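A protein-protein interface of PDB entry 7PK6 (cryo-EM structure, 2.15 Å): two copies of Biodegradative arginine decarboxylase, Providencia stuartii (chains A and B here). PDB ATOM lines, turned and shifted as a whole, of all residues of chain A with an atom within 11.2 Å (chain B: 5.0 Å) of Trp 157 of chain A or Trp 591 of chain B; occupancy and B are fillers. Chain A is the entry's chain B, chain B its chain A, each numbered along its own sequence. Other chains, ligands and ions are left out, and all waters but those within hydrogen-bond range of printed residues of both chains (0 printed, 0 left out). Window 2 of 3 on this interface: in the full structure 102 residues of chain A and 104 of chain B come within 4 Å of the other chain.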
ATOM      1  N   TYR A 149     -13.388  -5.612 -17.253  1.00  0.00           N
ATOM      2  CA  TYR A 149     -14.494  -4.723 -16.931  1.00  0.00           C
ATOM      3  C   TYR A 149     -15.277  -4.310 -18.173  1.00  0.00           C
ATOM      4  O   TYR A 149     -16.467  -4.004 -18.064  1.00  0.00           O
ATOM      5  CB  TYR A 149     -13.965  -3.501 -16.168  1.00  0.00           C
ATOM      6  CG  TYR A 149     -14.986  -2.430 -15.833  1.00  0.00           C
ATOM      7  CD1 TYR A 149     -15.414  -2.259 -14.525  1.00  0.00           C
ATOM      8  CD2 TYR A 149     -15.475  -1.558 -16.795  1.00  0.00           C
ATOM      9  CE1 TYR A 149     -16.336  -1.289 -14.194  1.00  0.00           C
ATOM     10  CE2 TYR A 149     -16.402  -0.592 -16.473  1.00  0.00           C
ATOM     11  CZ  TYR A 149     -16.822  -0.455 -15.172  1.00  0.00           C
ATOM     12  OH  TYR A 149     -17.735   0.519 -14.850  1.00  0.00           O
ATOM     13  N   VAL A 152     -19.030  -5.138 -18.989  1.00  0.00           N
ATOM     14  CA  VAL A 152     -20.157  -4.507 -18.312  1.00  0.00           C
ATOM     15  C   VAL A 152     -20.787  -3.476 -19.239  1.00  0.00           C
ATOM     16  O   VAL A 152     -20.088  -2.649 -19.839  1.00  0.00           O
ATOM     17  CB  VAL A 152     -19.699  -3.868 -16.994  1.00  0.00           C
ATOM     18  CG1 VAL A 152     -20.800  -3.000 -16.406  1.00  0.00           C
ATOM     19  CG2 VAL A 152     -19.272  -4.941 -16.006  1.00  0.00           C
ATOM     20  N   HIS A 153     -22.115  -3.522 -19.372  1.00  0.00           N
ATOM     21  CA  HIS A 153     -22.824  -2.598 -20.251  1.00  0.00           C
ATOM     22  C   HIS A 153     -23.931  -1.816 -19.557  1.00  0.00           C
ATOM     23  O   HIS A 153     -24.673  -1.095 -20.229  1.00  0.00           O
ATOM     24  CB  HIS A 153     -23.411  -3.335 -21.458  1.00  0.00           C
ATOM     25  CG  HIS A 153     -22.432  -4.218 -22.166  1.00  0.00           C
ATOM     26  ND1 HIS A 153     -21.133  -3.835 -22.420  1.00  0.00           N
ATOM     27  CD2 HIS A 153     -22.561  -5.467 -22.667  1.00  0.00           C
ATOM     28  CE1 HIS A 153     -20.504  -4.812 -23.049  1.00  0.00           C
ATOM     29  NE2 HIS A 153     -21.350  -5.813 -23.213  1.00  0.00           N
ATOM     30  N   GLU A 154     -24.057  -1.925 -18.241  1.00  0.00           N
ATOM     31  CA  GLU A 154     -25.150  -1.279 -17.535  1.00  0.00           C
ATOM     32  C   GLU A 154     -24.938   0.229 -17.462  1.00  0.00           C
ATOM     33  O   GLU A 154     -23.810   0.718 -17.361  1.00  0.00           O
ATOM     34  CB  GLU A 154     -25.298  -1.856 -16.125  1.00  0.00           C
ATOM     35  CG  GLU A 154     -24.136  -1.541 -15.192  1.00  0.00           C
ATOM     36  CD  GLU A 154     -23.835  -2.667 -14.215  1.00  0.00           C
ATOM     37  OE1 GLU A 154     -24.579  -3.668 -14.200  1.00  0.00           O
ATOM     38  OE2 GLU A 154     -22.844  -2.552 -13.465  1.00  0.00           O
ATOM     39  N   TYR A 155     -26.041   0.964 -17.522  1.00  0.00           N
ATOM     40  CA  TYR A 155     -26.012   2.413 -17.363  1.00  0.00           C
ATOM     41  C   TYR A 155     -25.642   2.749 -15.927  1.00  0.00           C
ATOM     42  O   TYR A 155     -26.451   2.597 -15.012  1.00  0.00           O
ATOM     43  CB  TYR A 155     -27.358   3.025 -17.730  1.00  0.00           C
ATOM     44  CG  TYR A 155     -27.420   4.521 -17.512  1.00  0.00           C
ATOM     45  CD1 TYR A 155     -26.960   5.402 -18.475  1.00  0.00           C
ATOM     46  CD2 TYR A 155     -27.940   5.050 -16.340  1.00  0.00           C
ATOM     47  CE1 TYR A 155     -27.011   6.761 -18.276  1.00  0.00           C
ATOM     48  CE2 TYR A 155     -27.996   6.410 -16.135  1.00  0.00           C
ATOM     49  CZ  TYR A 155     -27.529   7.262 -17.105  1.00  0.00           C
ATOM     50  OH  TYR A 155     -27.581   8.618 -16.907  1.00  0.00           O
ATOM     51  N   SER A 156     -24.410   3.191 -15.721  1.00  0.00           N
ATOM     52  CA  SER A 156     -24.089   3.875 -14.483  1.00  0.00           C
ATOM     53  C   SER A 156     -24.753   5.241 -14.497  1.00  0.00           C
ATOM     54  O   SER A 156     -25.020   5.813 -15.556  1.00  0.00           O
ATOM     55  CB  SER A 156     -22.580   4.025 -14.315  1.00  0.00           C
ATOM     56  OG  SER A 156     -22.070   5.016 -15.187  1.00  0.00           O
ATOM     57  N   TRP A 157     -25.024   5.767 -13.312  1.00  0.00           N
ATOM     58  CA  TRP A 157     -25.690   7.057 -13.186  1.00  0.00           C
ATOM     59  C   TRP A 157     -24.689   8.166 -12.906  1.00  0.00           C
ATOM     60  O   TRP A 157     -24.955   9.084 -12.128  1.00  0.00           O
ATOM     61  CB  TRP A 157     -26.770   6.982 -12.113  1.00  0.00           C
ATOM     62  CG  TRP A 157     -27.805   5.957 -12.462  1.00  0.00           C
ATOM     63  CD1 TRP A 157     -27.694   4.605 -12.334  1.00  0.00           C
ATOM     64  CD2 TRP A 157     -29.087   6.198 -13.045  1.00  0.00           C
ATOM     65  NE1 TRP A 157     -28.831   3.991 -12.783  1.00  0.00           N
ATOM     66  CE2 TRP A 157     -29.704   4.948 -13.227  1.00  0.00           C
ATOM     67  CE3 TRP A 157     -29.777   7.351 -13.426  1.00  0.00           C
ATOM     68  CZ2 TRP A 157     -30.978   4.817 -13.770  1.00  0.00           C
ATOM     69  CZ3 TRP A 157     -31.038   7.220 -13.966  1.00  0.00           C
ATOM     70  CH2 TRP A 157     -31.627   5.962 -14.134  1.00  0.00           C
ATOM     71  N   ALA A 158     -23.514   8.076 -13.528  1.00  0.00           N
ATOM     72  CA  ALA A 158     -22.423   9.013 -13.318  1.00  0.00           C
ATOM     73  C   ALA A 158     -21.712   9.265 -14.643  1.00  0.00           C
ATOM     74  O   ALA A 158     -22.001   8.631 -15.659  1.00  0.00           O
ATOM     75  CB  ALA A 158     -21.446   8.490 -12.262  1.00  0.00           C
ATOM     76  N   ALA A 159     -20.771  10.204 -14.621  1.00  0.00           N
ATOM     77  CA  ALA A 159     -19.994  10.536 -15.803  1.00  0.00           C
ATOM     78  C   ALA A 159     -18.994   9.420 -16.116  1.00  0.00           C
ATOM     79  O   ALA A 159     -18.641   8.631 -15.238  1.00  0.00           O
ATOM     80  CB  ALA A 159     -19.261  11.857 -15.588  1.00  0.00           C
ATOM     81  N   PRO A 160     -18.513   9.328 -17.370  1.00  0.00           N
ATOM     82  CA  PRO A 160     -18.780  10.178 -18.538  1.00  0.00           C
ATOM     83  C   PRO A 160     -20.184  10.016 -19.105  1.00  0.00           C
ATOM     84  O   PRO A 160     -20.787   8.955 -18.991  1.00  0.00           O
ATOM     85  CB  PRO A 160     -17.732   9.721 -19.559  1.00  0.00           C
ATOM     86  CG  PRO A 160     -17.336   8.377 -19.133  1.00  0.00           C
ATOM     87  CD  PRO A 160     -17.481   8.319 -17.654  1.00  0.00           C
ATOM     88  N   GLY A 161     -20.688  11.088 -19.716  1.00  0.00           N
ATOM     89  CA  GLY A 161     -22.061  11.118 -20.181  1.00  0.00           C
ATOM     90  C   GLY A 161     -22.361  10.185 -21.332  1.00  0.00           C
ATOM     91  O   GLY A 161     -23.506   9.749 -21.470  1.00  0.00           O
ATOM     92  N   HIS A 162     -21.367   9.866 -22.165  1.00  0.00           N
ATOM     93  CA  HIS A 162     -21.637   9.016 -23.318  1.00  0.00           C
ATOM     94  C   HIS A 162     -21.970   7.584 -22.919  1.00  0.00           C
ATOM     95  O   HIS A 162     -22.561   6.860 -23.722  1.00  0.00           O
ATOM     96  CB  HIS A 162     -20.461   9.047 -24.302  1.00  0.00           C
ATOM     97  CG  HIS A 162     -19.190   8.462 -23.769  1.00  0.00           C
ATOM     98  ND1 HIS A 162     -18.994   7.107 -23.629  1.00  0.00           N
ATOM     99  CD2 HIS A 162     -18.042   9.050 -23.363  1.00  0.00           C
ATOM    100  CE1 HIS A 162     -17.786   6.885 -23.147  1.00  0.00           C
ATOM    101  NE2 HIS A 162     -17.187   8.048 -22.977  1.00  0.00           N
ATOM    102  N   GLN A 163     -21.610   7.168 -21.703  1.00  0.00           N
ATOM    103  CA  GLN A 163     -22.030   5.889 -21.129  1.00  0.00           C
ATOM    104  C   GLN A 163     -21.619   4.709 -22.012  1.00  0.00           C
ATOM    105  O   GLN A 163     -22.450   3.968 -22.537  1.00  0.00           O
ATOM    106  CB  GLN A 163     -23.539   5.882 -20.867  1.00  0.00           C
ATOM    107  CG  GLN A 163     -23.984   6.941 -19.893  1.00  0.00           C
ATOM    108  CD  GLN A 163     -23.654   6.578 -18.464  1.00  0.00           C
ATOM    109  OE1 GLN A 163     -23.464   5.411 -18.139  1.00  0.00           O
ATOM    110  NE2 GLN A 163     -23.581   7.580 -17.604  1.00  0.00           N
ATOM    111  N   GLY A 164     -20.311   4.548 -22.168  1.00  0.00           N
ATOM    112  CA  GLY A 164     -19.797   3.462 -22.974  1.00  0.00           C
ATOM    113  C   GLY A 164     -20.076   3.592 -24.451  1.00  0.00           C
ATOM    114  O   GLY A 164     -20.177   2.580 -25.143  1.00  0.00           O
ATOM    115  N   ILE A 190     -14.320   4.826 -18.508  1.00  0.00           N
ATOM    116  CA  ILE A 190     -15.251   4.470 -17.444  1.00  0.00           C
ATOM    117  C   ILE A 190     -15.238   5.443 -16.279  1.00  0.00           C
ATOM    118  O   ILE A 190     -16.114   5.345 -15.408  1.00  0.00           O
ATOM    119  CB  ILE A 190     -14.990   3.041 -16.929  1.00  0.00           C
ATOM    120  CG1 ILE A 190     -13.594   2.945 -16.316  1.00  0.00           C
ATOM    121  CG2 ILE A 190     -15.116   2.061 -18.066  1.00  0.00           C
ATOM    122  CD1 ILE A 190     -13.244   1.569 -15.811  1.00  0.00           C
ATOM    123  N   GLY A 191     -14.298   6.373 -16.230  1.00  0.00           N
ATOM    124  CA  GLY A 191     -14.197   7.253 -15.088  1.00  0.00           C
ATOM    125  C   GLY A 191     -13.349   6.657 -13.986  1.00  0.00           C
ATOM    126  O   GLY A 191     -12.937   5.495 -14.019  1.00  0.00           O
ATOM    127  N   GLU A 193     -14.202   6.246 -10.818  1.00  0.00           N
ATOM    128  CA  GLU A 193     -15.040   5.851  -9.690  1.00  0.00           C
ATOM    129  C   GLU A 193     -15.451   4.382  -9.745  1.00  0.00           C
ATOM    130  O   GLU A 193     -16.410   3.981  -9.084  1.00  0.00           O
ATOM    131  CB  GLU A 193     -16.284   6.733  -9.613  1.00  0.00           C
ATOM    132  CG  GLU A 193     -16.254   7.738  -8.482  1.00  0.00           C
ATOM    133  CD  GLU A 193     -15.205   8.805  -8.692  1.00  0.00           C
ATOM    134  OE1 GLU A 193     -14.493   9.144  -7.722  1.00  0.00           O
ATOM    135  OE2 GLU A 193     -15.100   9.310  -9.828  1.00  0.00           O
ATOM    136  N   ARG A 194     -14.745   3.569 -10.522  1.00  0.00           N
ATOM    137  CA  ARG A 194     -15.026   2.140 -10.607  1.00  0.00           C
ATOM    138  C   ARG A 194     -13.937   1.401  -9.843  1.00  0.00           C
ATOM    139  O   ARG A 194     -12.811   1.264 -10.332  1.00  0.00           O
ATOM    140  CB  ARG A 194     -15.110   1.677 -12.059  1.00  0.00           C
ATOM    141  CG  ARG A 194     -15.774   2.676 -12.994  1.00  0.00           C
ATOM    142  CD  ARG A 194     -17.242   2.905 -12.658  1.00  0.00           C
ATOM    143  NE  ARG A 194     -17.863   1.740 -12.037  1.00  0.00           N
ATOM    144  CZ  ARG A 194     -19.084   1.735 -11.516  1.00  0.00           C
ATOM    145  NH1 ARG A 194     -19.823   2.836 -11.544  1.00  0.00           N
ATOM    146  NH2 ARG A 194     -19.571   0.629 -10.968  1.00  0.00           N
ATOM    147  N   GLU B 453     -36.791  12.400 -19.461  1.00  0.00           N
ATOM    148  CA  GLU B 453     -36.531  11.218 -18.641  1.00  0.00           C
ATOM    149  C   GLU B 453     -36.405  11.583 -17.165  1.00  0.00           C
ATOM    150  O   GLU B 453     -36.978  10.909 -16.294  1.00  0.00           O
ATOM    151  CB  GLU B 453     -35.269  10.504 -19.121  1.00  0.00           C
ATOM    152  CG  GLU B 453     -35.425   9.773 -20.439  1.00  0.00           C
ATOM    153  CD  GLU B 453     -36.390   8.609 -20.354  1.00  0.00           C
ATOM    154  OE1 GLU B 453     -37.406   8.619 -21.077  1.00  0.00           O
ATOM    155  OE2 GLU B 453     -36.132   7.681 -19.561  1.00  0.00           O
ATOM    156  N   ASP B 456     -39.859  12.386 -15.768  1.00  0.00           N
ATOM    157  CA  ASP B 456     -40.637  11.174 -15.540  1.00  0.00           C
ATOM    158  C   ASP B 456     -40.207  10.487 -14.254  1.00  0.00           C
ATOM    159  O   ASP B 456     -41.052  10.073 -13.449  1.00  0.00           O
ATOM    160  CB  ASP B 456     -40.498  10.221 -16.725  1.00  0.00           C
ATOM    161  CG  ASP B 456     -41.280  10.679 -17.938  1.00  0.00           C
ATOM    162  OD1 ASP B 456     -42.089  11.619 -17.809  1.00  0.00           O
ATOM    163  OD2 ASP B 456     -41.080  10.105 -19.026  1.00  0.00           O
ATOM    164  N   PHE B 457     -38.894  10.386 -14.027  1.00  0.00           N
ATOM    165  CA  PHE B 457     -38.420   9.788 -12.784  1.00  0.00           C
ATOM    166  C   PHE B 457     -38.872  10.592 -11.567  1.00  0.00           C
ATOM    167  O   PHE B 457     -39.344  10.017 -10.579  1.00  0.00           O
ATOM    168  CB  PHE B 457     -36.900   9.662 -12.800  1.00  0.00           C
ATOM    169  CG  PHE B 457     -36.330   9.143 -11.517  1.00  0.00           C
ATOM    170  CD1 PHE B 457     -36.658   7.881 -11.064  1.00  0.00           C
ATOM    171  CD2 PHE B 457     -35.476   9.918 -10.760  1.00  0.00           C
ATOM    172  CE1 PHE B 457     -36.142   7.401  -9.884  1.00  0.00           C
ATOM    173  CE2 PHE B 457     -34.956   9.441  -9.579  1.00  0.00           C
ATOM    174  CZ  PHE B 457     -35.291   8.180  -9.141  1.00  0.00           C
ATOM    175  N   SER B 460     -42.692  10.140 -10.977  1.00  0.00           N
ATOM    176  CA  SER B 460     -43.002   8.804 -10.482  1.00  0.00           C
ATOM    177  C   SER B 460     -42.588   8.645  -9.028  1.00  0.00           C
ATOM    178  O   SER B 460     -43.325   8.059  -8.223  1.00  0.00           O
ATOM    179  CB  SER B 460     -42.321   7.753 -11.352  1.00  0.00           C
ATOM    180  OG  SER B 460     -42.961   7.652 -12.607  1.00  0.00           O
ATOM    181  N   ILE B 568     -25.380   0.571  -8.976  1.00  0.00           N
ATOM    182  CA  ILE B 568     -25.639   1.999  -9.114  1.00  0.00           C
ATOM    183  C   ILE B 568     -24.702   2.756  -8.184  1.00  0.00           C
ATOM    184  O   ILE B 568     -24.649   2.485  -6.980  1.00  0.00           O
ATOM    185  CB  ILE B 568     -27.108   2.316  -8.808  1.00  0.00           C
ATOM    186  CG1 ILE B 568     -28.018   1.614  -9.814  1.00  0.00           C
ATOM    187  CG2 ILE B 568     -27.346   3.812  -8.813  1.00  0.00           C
ATOM    188  CD1 ILE B 568     -29.167   0.874  -9.184  1.00  0.00           C
ATOM    189  N   VAL B 569     -23.948   3.698  -8.736  1.00  0.00           N
ATOM    190  CA  VAL B 569     -23.008   4.489  -7.951  1.00  0.00           C
ATOM    191  C   VAL B 569     -23.441   5.951  -8.033  1.00  0.00           C
ATOM    192  O   VAL B 569     -23.320   6.575  -9.097  1.00  0.00           O
ATOM    193  CB  VAL B 569     -21.565   4.305  -8.430  1.00  0.00           C
ATOM    194  CG1 VAL B 569     -20.622   5.110  -7.555  1.00  0.00           C
ATOM    195  CG2 VAL B 569     -21.187   2.836  -8.401  1.00  0.00           C
ATOM    196  N   THR B 571     -23.467  10.065  -7.661  1.00  0.00           N
ATOM    197  CA  THR B 571     -22.452  11.095  -7.849  1.00  0.00           C
ATOM    198  C   THR B 571     -22.142  11.826  -6.547  1.00  0.00           C
ATOM    199  O   THR B 571     -20.974  12.061  -6.223  1.00  0.00           O
ATOM    200  CB  THR B 571     -22.913  12.086  -8.919  1.00  0.00           C
ATOM    201  OG1 THR B 571     -23.738  11.412  -9.875  1.00  0.00           O
ATOM    202  CG2 THR B 571     -21.722  12.709  -9.627  1.00  0.00           C
ATOM    203  N   PHE B 580     -28.421  11.398  -8.446  1.00  0.00           N
ATOM    204  CA  PHE B 580     -28.311  10.564  -9.633  1.00  0.00           C
ATOM    205  C   PHE B 580     -28.173  11.449 -10.861  1.00  0.00           C
ATOM    206  O   PHE B 580     -28.854  12.469 -10.983  1.00  0.00           O
ATOM    207  CB  PHE B 580     -29.528   9.652  -9.800  1.00  0.00           C
ATOM    208  CG  PHE B 580     -29.729   8.702  -8.668  1.00  0.00           C
ATOM    209  CD1 PHE B 580     -29.068   7.489  -8.642  1.00  0.00           C
ATOM    210  CD2 PHE B 580     -30.579   9.018  -7.628  1.00  0.00           C
ATOM    211  CE1 PHE B 580     -29.252   6.613  -7.598  1.00  0.00           C
ATOM    212  CE2 PHE B 580     -30.766   8.145  -6.584  1.00  0.00           C
ATOM    213  CZ  PHE B 580     -30.103   6.940  -6.571  1.00  0.00           C
ATOM    214  N   LEU B 581     -27.298  11.049 -11.773  1.00  0.00           N
ATOM    215  CA  LEU B 581     -27.055  11.787 -13.001  1.00  0.00           C
ATOM    216  C   LEU B 581     -27.873  11.197 -14.137  1.00  0.00           C
ATOM    217  O   LEU B 581     -27.817   9.991 -14.388  1.00  0.00           O
ATOM    218  CB  LEU B 581     -25.573  11.759 -13.367  1.00  0.00           C
ATOM    219  CG  LEU B 581     -24.917  13.068 -13.783  1.00  0.00           C
ATOM    220  CD1 LEU B 581     -24.919  14.046 -12.634  1.00  0.00           C
ATOM    221  CD2 LEU B 581     -23.507  12.793 -14.252  1.00  0.00           C
ATOM    222  N   PHE B 582     -28.630  12.045 -14.815  1.00  0.00           N
ATOM    223  CA  PHE B 582     -29.262  11.700 -16.079  1.00  0.00           C
ATOM    224  C   PHE B 582     -28.457  12.367 -17.185  1.00  0.00           C
ATOM    225  O   PHE B 582     -28.333  13.595 -17.209  1.00  0.00           O
ATOM    226  CB  PHE B 582     -30.721  12.157 -16.113  1.00  0.00           C
ATOM    227  CG  PHE B 582     -31.654  11.286 -15.322  1.00  0.00           C
ATOM    228  CD1 PHE B 582     -31.516  11.160 -13.951  1.00  0.00           C
ATOM    229  CD2 PHE B 582     -32.677  10.601 -15.948  1.00  0.00           C
ATOM    230  CE1 PHE B 582     -32.375  10.362 -13.227  1.00  0.00           C
ATOM    231  CE2 PHE B 582     -33.538   9.803 -15.226  1.00  0.00           C
ATOM    232  CZ  PHE B 582     -33.387   9.684 -13.865  1.00  0.00           C
ATOM    233  N   ILE B 586     -28.175   8.024 -21.419  1.00  0.00           N
ATOM    234  CA  ILE B 586     -29.221   7.197 -20.830  1.00  0.00           C
ATOM    235  C   ILE B 586     -30.207   6.782 -21.912  1.00  0.00           C
ATOM    236  O   ILE B 586     -30.374   7.459 -22.930  1.00  0.00           O
ATOM    237  CB  ILE B 586     -29.927   7.938 -19.677  1.00  0.00           C
ATOM    238  CG1 ILE B 586     -30.538   6.937 -18.696  1.00  0.00           C
ATOM    239  CG2 ILE B 586     -30.995   8.882 -20.207  1.00  0.00           C
ATOM    240  CD1 ILE B 586     -31.141   7.580 -17.478  1.00  0.00           C
ATOM    241  N   GLY B 589     -36.796   5.028 -20.228  1.00  0.00           N
ATOM    242  CA  GLY B 589     -37.354   4.092 -19.276  1.00  0.00           C
ATOM    243  C   GLY B 589     -36.356   3.431 -18.355  1.00  0.00           C
ATOM    244  O   GLY B 589     -36.735   2.518 -17.618  1.00  0.00           O
ATOM    245  N   LYS B 590     -35.094   3.863 -18.374  1.00  0.00           N
ATOM    246  CA  LYS B 590     -34.066   3.240 -17.548  1.00  0.00           C
ATOM    247  C   LYS B 590     -34.289   3.499 -16.061  1.00  0.00           C
ATOM    248  O   LYS B 590     -33.877   2.687 -15.228  1.00  0.00           O
ATOM    249  CB  LYS B 590     -32.686   3.746 -17.979  1.00  0.00           C
ATOM    250  CG  LYS B 590     -31.510   3.113 -17.261  1.00  0.00           C
ATOM    251  CD  LYS B 590     -31.522   1.602 -17.382  1.00  0.00           C
ATOM    252  CE  LYS B 590     -30.284   0.993 -16.753  1.00  0.00           C
ATOM    253  NZ  LYS B 590     -30.529  -0.369 -16.207  1.00  0.00           N
ATOM    254  N   TRP B 591     -34.944   4.607 -15.709  1.00  0.00           N
ATOM    255  CA  TRP B 591     -35.177   4.949 -14.309  1.00  0.00           C
ATOM    256  C   TRP B 591     -36.111   3.970 -13.604  1.00  0.00           C
ATOM    257  O   TRP B 591     -36.208   4.004 -12.369  1.00  0.00           O
ATOM    258  CB  TRP B 591     -35.728   6.373 -14.211  1.00  0.00           C
ATOM    259  CG  TRP B 591     -36.950   6.604 -15.039  1.00  0.00           C
ATOM    260  CD1 TRP B 591     -36.996   7.095 -16.306  1.00  0.00           C
ATOM    261  CD2 TRP B 591     -38.305   6.343 -14.661  1.00  0.00           C
ATOM    262  NE1 TRP B 591     -38.292   7.161 -16.741  1.00  0.00           N
ATOM    263  CE2 TRP B 591     -39.117   6.704 -15.750  1.00  0.00           C
ATOM    264  CE3 TRP B 591     -38.909   5.840 -13.507  1.00  0.00           C
ATOM    265  CZ2 TRP B 591     -40.501   6.582 -15.719  1.00  0.00           C
ATOM    266  CZ3 TRP B 591     -40.281   5.716 -13.481  1.00  0.00           C
ATOM    267  CH2 TRP B 591     -41.062   6.085 -14.578  1.00  0.00           C
ATOM    268  N   GLY B 592     -36.797   3.109 -14.355  1.00  0.00           N
ATOM    269  CA  GLY B 592     -37.575   2.056 -13.730  1.00  0.00           C
ATOM    270  C   GLY B 592     -36.724   1.127 -12.886  1.00  0.00           C
ATOM    271  O   GLY B 592     -37.167   0.647 -11.843  1.00  0.00           O
ATOM    272  N   THR B 593     -35.489   0.863 -13.325  1.00  0.00           N
ATOM    273  CA  THR B 593     -34.565   0.081 -12.507  1.00  0.00           C
ATOM    274  C   THR B 593     -34.281   0.773 -11.184  1.00  0.00           C
ATOM    275  O   THR B 593     -34.239   0.125 -10.135  1.00  0.00           O
ATOM    276  CB  THR B 593     -33.253  -0.161 -13.256  1.00  0.00           C
ATOM    277  OG1 THR B 593     -33.491  -1.019 -14.373  1.00  0.00           O
ATOM    278  CG2 THR B 593     -32.225  -0.810 -12.351  1.00  0.00           C
ATOM    279  N   LEU B 594     -34.066   2.087 -11.219  1.00  0.00           N
ATOM    280  CA  LEU B 594     -33.813   2.831  -9.992  1.00  0.00           C
ATOM    281  C   LEU B 594     -34.999   2.744  -9.044  1.00  0.00           C
ATOM    282  O   LEU B 594     -34.833   2.509  -7.839  1.00  0.00           O
ATOM    283  CB  LEU B 594     -33.502   4.285 -10.337  1.00  0.00           C
ATOM    284  CG  LEU B 594     -32.653   5.079  -9.355  1.00  0.00           C
ATOM    285  CD1 LEU B 594     -31.470   4.244  -8.916  1.00  0.00           C
ATOM    286  CD2 LEU B 594     -32.199   6.377  -9.997  1.00  0.00           C
ATOM    287  N   VAL B 595     -36.208   2.919  -9.578  1.00  0.00           N
ATOM    288  CA  VAL B 595     -37.407   2.832  -8.750  1.00  0.00           C
ATOM    289  C   VAL B 595     -37.547   1.434  -8.157  1.00  0.00           C
ATOM    290  O   VAL B 595     -37.859   1.272  -6.970  1.00  0.00           O
ATOM    291  CB  VAL B 595     -38.649   3.229  -9.567  1.00  0.00           C
ATOM    292  CG1 VAL B 595     -39.908   2.933  -8.788  1.00  0.00           C
ATOM    293  CG2 VAL B 595     -38.584   4.696  -9.942  1.00  0.00           C
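O of Trp 157 of chain A is in hydrogen-bond range of OG1 of Thr 571 of chain B (3.5 Å).
O of Leu 581 of chain B lies within hydrogen-bond range of OH of Tyr 155 of chain A (2.9 Å).
N of Leu 581 of chain B sits close to O of Trp 157 of chain A (3.1 Å).
NE of Arg 194 of chain A lies within hydrogen-bond range of OH of Tyr 149 of chain A, 3.1 Å away.
The backbone carbonyl oxygen of Ala 158 of chain A lies within hydrogen-bond range of the side-chain amide nitrogen of Gln 163 of chain A, at 2.7 Å.
Among the printed residues, pairs that only touch across the chains: Tyr 155 of chain A with Phe 582 of chain B (3.6 Å), Tyr 155 of chain A with Ile 586 of chain B (3.4 Å), Tyr 155 of chain A with Lys 590 of chain B (3.7 Å), Trp 157 of chain A with Ile 568 of chain B (3.6 Å), Trp 157 of chain A with Phe 582 of chain B (3.4 Å), Trp 157 of chain A with Ile 586 of chain B (3.5 Å), Trp 157 of chain A with Lys 590 of chain B (3.9 Å), Trp 157 of chain A with Trp 591 of chain B (3.7 Å), Ala 158 of chain A with Leu 581 of chain B (3.98 Å), Ala 159 of chain A with Leu 581 of chain B (3.8 Å) and Arg 194 of chain A with Val 569 of chain B (3.4 Å).
Trp 157 of chain A touches just these residues of chain B: Ile 568 (3.6 Å), Thr 571 (3.5 Å), Leu 581 (3.0 Å), Phe 582 (3.4 Å), Ile 586 (3.5 Å), Lys 590 (3.9 Å) and Trp 591 (3.7 Å).
Of the printed residues of chain B, Ala 159 of chain A touches Leu 581.
Of the printed residues of chain B, Arg 194 of chain A touches Val 569.
No residue of chain A comes within 4 Å of Glu 453 of chain B.
Asp 456 of chain B touches none of the printed residues of chain A.
No residue of chain A comes within 4 Å of Phe 457 of chain B.
No residue of chain A comes within 4 Å of Ser 460 of chain B.
Of chain A, only Trp 157 (3.6 Å) comes within 4 Å of Ile 568 of chain B.
Leu 581 of chain B touches just these residues of chain A: Tyr 155, Trp 157, Ala 158 and Ala 159.
Lys 590 of chain B touches two residues of chain A.
Trp 591 of chain B touches just one residue of chain A: Trp 157.
Gly 592 of chain B touches none of the printed residues of chain A.
Thr 593 of chain B touches none of the printed residues of chain A.
No residue of chain A comes within 4 Å of Val 595 of chain B.
The nearest printed residue of chain B that does not touch Trp 157 of chain A is Phe 580 of chain B (4.2 Å).
The nearest residue of chain A that does not touch Trp 591 of chain B is Tyr 155 of chain A (7.0 Å).
The nearest printed residue of chain A that does not touch Val 569 of chain B is Ala 158 of chain A (4.1 Å).
Hydrophobic or aromatic side chains of chain B that line the printed part of chain A: Ile 568, Val 569, Leu 581, Phe 582 and Ile 586.
Along chain B the printed residues that touch a printed residue of chain A span positions 568 to 591.
Hydrophobic or aromatic side chains of chain A that line the printed part of chain B: Tyr 155 and Trp 157.
Among the printed residues, 14 pairs touch across the chains.
No position is printed for both chains.
Of the 14 pairs that touch across the chains among the printed residues, none has its exchanged pair printed and touching as well.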
